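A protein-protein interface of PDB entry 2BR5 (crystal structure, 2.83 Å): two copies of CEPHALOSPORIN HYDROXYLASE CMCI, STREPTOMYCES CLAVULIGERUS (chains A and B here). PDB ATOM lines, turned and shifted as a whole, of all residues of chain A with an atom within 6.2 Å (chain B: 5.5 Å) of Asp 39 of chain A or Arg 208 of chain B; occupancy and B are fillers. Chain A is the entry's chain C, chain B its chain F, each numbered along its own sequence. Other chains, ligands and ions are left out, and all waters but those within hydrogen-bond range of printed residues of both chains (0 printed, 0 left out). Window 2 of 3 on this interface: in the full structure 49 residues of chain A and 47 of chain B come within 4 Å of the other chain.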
ATOM      1  N   PRO A  37       1.222  25.516   4.007  1.00  0.00           N
ATOM      2  CA  PRO A  37       1.728  25.247   5.349  1.00  0.00           C
ATOM      3  C   PRO A  37       0.596  25.159   6.357  1.00  0.00           C
ATOM      4  O   PRO A  37      -0.251  26.044   6.415  1.00  0.00           O
ATOM      5  CB  PRO A  37       2.618  26.452   5.628  1.00  0.00           C
ATOM      6  CG  PRO A  37       2.013  27.551   4.834  1.00  0.00           C
ATOM      7  CD  PRO A  37       1.500  26.898   3.587  1.00  0.00           C
ATOM      8  N   LEU A  38       0.600  24.087   7.139  1.00  0.00           N
ATOM      9  CA  LEU A  38      -0.490  23.791   8.070  1.00  0.00           C
ATOM     10  C   LEU A  38      -0.669  24.814   9.206  1.00  0.00           C
ATOM     11  O   LEU A  38      -1.771  24.960   9.732  1.00  0.00           O
ATOM     12  CB  LEU A  38      -0.310  22.383   8.642  1.00  0.00           C
ATOM     13  CG  LEU A  38      -1.160  21.272   8.008  1.00  0.00           C
ATOM     14  CD1 LEU A  38      -1.350  21.452   6.507  1.00  0.00           C
ATOM     15  CD2 LEU A  38      -0.588  19.874   8.326  1.00  0.00           C
ATOM     16  N   ASP A  39       0.396  25.521   9.589  1.00  0.00           N
ATOM     17  CA  ASP A  39       0.267  26.579  10.603  1.00  0.00           C
ATOM     18  C   ASP A  39      -0.562  27.762  10.114  1.00  0.00           C
ATOM     19  O   ASP A  39      -1.069  28.530  10.917  1.00  0.00           O
ATOM     20  CB  ASP A  39       1.629  27.046  11.156  1.00  0.00           C
ATOM     21  CG  ASP A  39       2.527  27.701  10.107  1.00  0.00           C
ATOM     22  OD1 ASP A  39       2.902  27.036   9.116  1.00  0.00           O
ATOM     23  OD2 ASP A  39       2.951  28.868  10.220  1.00  0.00           O
ATOM     24  N   ARG A  40      -0.710  27.895   8.801  1.00  0.00           N
ATOM     25  CA  ARG A  40      -1.597  28.895   8.224  1.00  0.00           C
ATOM     26  C   ARG A  40      -2.790  28.226   7.516  1.00  0.00           C
ATOM     27  O   ARG A  40      -3.372  28.789   6.592  1.00  0.00           O
ATOM     28  CB  ARG A  40      -0.815  29.805   7.263  1.00  0.00           C
ATOM     29  CG  ARG A  40       0.389  30.516   7.895  1.00  0.00           C
ATOM     30  CD  ARG A  40       1.067  31.560   6.999  1.00  0.00           C
ATOM     31  NE  ARG A  40       0.095  32.427   6.317  1.00  0.00           N
ATOM     32  CZ  ARG A  40       0.150  32.826   5.035  1.00  0.00           C
ATOM     33  NH1 ARG A  40       1.148  32.467   4.225  1.00  0.00           N
ATOM     34  NH2 ARG A  40      -0.815  33.601   4.554  1.00  0.00           N
ATOM     35  N   TRP A  41      -3.179  27.046   7.983  1.00  0.00           N
ATOM     36  CA  TRP A  41      -4.308  26.315   7.410  1.00  0.00           C
ATOM     37  C   TRP A  41      -5.564  27.159   7.068  1.00  0.00           C
ATOM     38  O   TRP A  41      -6.105  27.042   5.963  1.00  0.00           O
ATOM     39  CB  TRP A  41      -4.708  25.177   8.355  1.00  0.00           C
ATOM     40  CG  TRP A  41      -5.843  24.330   7.857  1.00  0.00           C
ATOM     41  CD1 TRP A  41      -5.752  23.250   7.039  1.00  0.00           C
ATOM     42  CD2 TRP A  41      -7.234  24.499   8.142  1.00  0.00           C
ATOM     43  NE1 TRP A  41      -7.000  22.728   6.796  1.00  0.00           N
ATOM     44  CE2 TRP A  41      -7.930  23.477   7.461  1.00  0.00           C
ATOM     45  CE3 TRP A  41      -7.968  25.415   8.900  1.00  0.00           C
ATOM     46  CZ2 TRP A  41      -9.313  23.336   7.526  1.00  0.00           C
ATOM     47  CZ3 TRP A  41      -9.344  25.276   8.961  1.00  0.00           C
ATOM     48  CH2 TRP A  41     -10.003  24.243   8.278  1.00  0.00           C
ATOM     49  N   ALA A  42      -6.037  27.973   8.011  1.00  0.00           N
ATOM     50  CA  ALA A  42      -7.305  28.698   7.842  1.00  0.00           C
ATOM     51  C   ALA A  42      -7.275  29.767   6.735  1.00  0.00           C
ATOM     52  O   ALA A  42      -8.289  29.999   6.081  1.00  0.00           O
ATOM     53  CB  ALA A  42      -7.749  29.317   9.160  1.00  0.00           C
ATOM     54  N   GLU A  43      -6.115  30.396   6.520  1.00  0.00           N
ATOM     55  CA  GLU A  43      -5.952  31.449   5.493  1.00  0.00           C
ATOM     56  C   GLU A  43      -5.808  30.939   4.054  1.00  0.00           C
ATOM     57  O   GLU A  43      -5.678  31.741   3.133  1.00  0.00           O
ATOM     58  CB  GLU A  43      -4.733  32.340   5.802  1.00  0.00           C
ATOM     59  CG  GLU A  43      -4.867  33.197   7.042  1.00  0.00           C
ATOM     60  CD  GLU A  43      -3.593  33.231   7.862  1.00  0.00           C
ATOM     61  OE1 GLU A  43      -2.736  34.108   7.593  1.00  0.00           O
ATOM     62  OE2 GLU A  43      -3.453  32.378   8.775  1.00  0.00           O
ATOM     63  N   LEU B 204      -3.596  21.270  14.204  1.00  0.00           N
ATOM     64  CA  LEU B 204      -3.109  21.130  12.836  1.00  0.00           C
ATOM     65  C   LEU B 204      -1.770  21.849  12.637  1.00  0.00           C
ATOM     66  O   LEU B 204      -0.899  21.363  11.914  1.00  0.00           O
ATOM     67  CB  LEU B 204      -4.124  21.687  11.837  1.00  0.00           C
ATOM     68  CG  LEU B 204      -4.739  20.679  10.876  1.00  0.00           C
ATOM     69  CD1 LEU B 204      -5.602  21.416   9.898  1.00  0.00           C
ATOM     70  CD2 LEU B 204      -3.667  19.904  10.160  1.00  0.00           C
ATOM     71  N   GLY B 205      -1.609  23.003  13.277  1.00  0.00           N
ATOM     72  CA  GLY B 205      -0.374  23.760  13.196  1.00  0.00           C
ATOM     73  C   GLY B 205       0.793  23.110  13.928  1.00  0.00           C
ATOM     74  O   GLY B 205       1.933  23.560  13.803  1.00  0.00           O
ATOM     75  N   ALA B 206       0.515  22.065  14.705  1.00  0.00           N
ATOM     76  CA  ALA B 206       1.560  21.323  15.400  1.00  0.00           C
ATOM     77  C   ALA B 206       2.341  20.453  14.409  1.00  0.00           C
ATOM     78  O   ALA B 206       3.512  20.117  14.645  1.00  0.00           O
ATOM     79  CB  ALA B 206       0.947  20.465  16.500  1.00  0.00           C
ATOM     80  N   PHE B 207       1.685  20.097  13.301  1.00  0.00           N
ATOM     81  CA  PHE B 207       2.301  19.280  12.258  1.00  0.00           C
ATOM     82  C   PHE B 207       2.862  20.118  11.128  1.00  0.00           C
ATOM     83  O   PHE B 207       3.160  19.574  10.079  1.00  0.00           O
ATOM     84  CB  PHE B 207       1.290  18.302  11.655  1.00  0.00           C
ATOM     85  CG  PHE B 207       0.696  17.351  12.643  1.00  0.00           C
ATOM     86  CD1 PHE B 207      -0.333  17.760  13.490  1.00  0.00           C
ATOM     87  CD2 PHE B 207       1.144  16.047  12.717  1.00  0.00           C
ATOM     88  CE1 PHE B 207      -0.897  16.886  14.393  1.00  0.00           C
ATOM     89  CE2 PHE B 207       0.594  15.177  13.612  1.00  0.00           C
ATOM     90  CZ  PHE B 207      -0.435  15.594  14.455  1.00  0.00           C
ATOM     91  N   ARG B 208       3.015  21.424  11.325  1.00  0.00           N
ATOM     92  CA  ARG B 208       3.483  22.291  10.252  1.00  0.00           C
ATOM     93  C   ARG B 208       4.759  21.770   9.605  1.00  0.00           C
ATOM     94  O   ARG B 208       4.926  21.888   8.420  1.00  0.00           O
ATOM     95  CB  ARG B 208       3.674  23.734  10.742  1.00  0.00           C
ATOM     96  CG  ARG B 208       5.055  24.054  11.329  1.00  0.00           C
ATOM     97  CD  ARG B 208       5.071  24.362  12.805  1.00  0.00           C
ATOM     98  NE  ARG B 208       4.304  25.567  13.088  1.00  0.00           N
ATOM     99  CZ  ARG B 208       4.276  26.179  14.264  1.00  0.00           C
ATOM    100  NH1 ARG B 208       4.996  25.716  15.296  1.00  0.00           N
ATOM    101  NH2 ARG B 208       3.527  27.271  14.406  1.00  0.00           N
ATOM    102  N   ASP B 209       5.649  21.173  10.386  1.00  0.00           N
ATOM    103  CA  ASP B 209       6.972  20.779   9.892  1.00  0.00           C
ATOM    104  C   ASP B 209       6.993  19.406   9.214  1.00  0.00           C
ATOM    105  O   ASP B 209       8.044  18.969   8.744  1.00  0.00           O
ATOM    106  CB  ASP B 209       7.989  20.793  11.052  1.00  0.00           C
ATOM    107  CG  ASP B 209       8.297  22.207  11.562  1.00  0.00           C
ATOM    108  OD1 ASP B 209       8.016  23.177  10.833  1.00  0.00           O
ATOM    109  OD2 ASP B 209       8.837  22.447  12.676  1.00  0.00           O
ATOM    110  N   VAL B 210       5.852  18.717   9.178  1.00  0.00           N
ATOM    111  CA  VAL B 210       5.796  17.321   8.695  1.00  0.00           C
ATOM    112  C   VAL B 210       4.739  17.087   7.630  1.00  0.00           C
ATOM    113  O   VAL B 210       4.998  16.377   6.670  1.00  0.00           O
ATOM    114  CB  VAL B 210       5.586  16.296   9.837  1.00  0.00           C
ATOM    115  CG1 VAL B 210       6.938  15.858  10.407  1.00  0.00           C
ATOM    116  CG2 VAL B 210       4.673  16.847  10.935  1.00  0.00           C
ATOM    117  N   LEU B 211       3.559  17.678   7.802  1.00  0.00           N
ATOM    118  CA  LEU B 211       2.489  17.589   6.811  1.00  0.00           C
ATOM    119  C   LEU B 211       2.125  18.953   6.217  1.00  0.00           C
ATOM    120  O   LEU B 211       2.252  19.988   6.867  1.00  0.00           O
ATOM    121  CB  LEU B 211       1.236  16.955   7.428  1.00  0.00           C
ATOM    122  CG  LEU B 211       1.394  15.544   7.982  1.00  0.00           C
ATOM    123  CD1 LEU B 211       0.249  15.239   8.939  1.00  0.00           C
ATOM    124  CD2 LEU B 211       1.470  14.525   6.856  1.00  0.00           C
ATOM    125  N   VAL B 232       6.171  15.905   4.002  1.00  0.00           N
ATOM    126  CA  VAL B 232       6.970  16.810   3.171  1.00  0.00           C
ATOM    127  C   VAL B 232       8.484  16.575   3.232  1.00  0.00           C
ATOM    128  O   VAL B 232       9.158  16.766   2.212  1.00  0.00           O
ATOM    129  CB  VAL B 232       6.648  18.319   3.422  1.00  0.00           C
ATOM    130  CG1 VAL B 232       5.482  18.505   4.368  1.00  0.00           C
ATOM    131  CG2 VAL B 232       7.867  19.101   3.940  1.00  0.00           C
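The backbone carbonyl oxygen of Gly 205 of chain B sits at hydrogen-bond distance from the guanidinium group of Arg 208 of chain B (3.2 Å).
Leu 204 of chain B touches Leu 38 of chain A. O of Leu 38 of chain A touches CA of Gly 205 of chain B, 3.9 Å away. Leu 38 of chain A touches Leu 211 of chain B. CA of Asp 39 of chain A touches CA of Gly 205 of chain B, at 3.9 Å. Arg 208 of chain B touches Asp 39 of chain A (NE to CB, 3.6 Å). CD1 of Leu 204 of chain B touches CD1 of Trp 41 of chain A, 3.4 Å away.
Of chain B, only Gly 205 and Arg 208 come within 4 Å of Asp 39 of chain A. Arg 208 of chain B touches one residue of chain A. Of the printed residues of chain B, Trp 41 of chain A touches Leu 204. Printed residues of chain A within 4 Å of Gly 205 of chain B: Leu 38 and Asp 39. Of the printed residues of chain B, Leu 38 of chain A touches Leu 204, Gly 205 and Leu 211. Printed residues of chain A within 4 Å of Leu 204 of chain B: Leu 38 (3.5 Å) and Trp 41 (3.4 Å). Val 232 of chain B touches none of the printed residues of chain A. The nearest residue of chain B that does not touch Asp 39 of chain A is Leu 204 of chain B (4.9 Å).
Of the 9 printed residues of chain B, 4 touch a printed residue of chain A. Printed residues of chain B that touch a printed residue of chain A: Leu 204, Gly 205, Arg 208 and Leu 211. Hydrophobic or aromatic side chains of chain B that line the printed part of chain A: Leu 204 and Leu 211. Of the 7 printed residues of chain A, 3 touch a printed residue of chain B. Hydrophobic or aromatic side chains of chain A within 4 Å of the printed part of chain B: Leu 38 and Trp 41. Among the printed residues, 6 pairs touch across the chains.
No position is printed for both chains. Of the 6 pairs that touch across the chains among the printed residues, none has its exchanged pair printed and touching as well.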
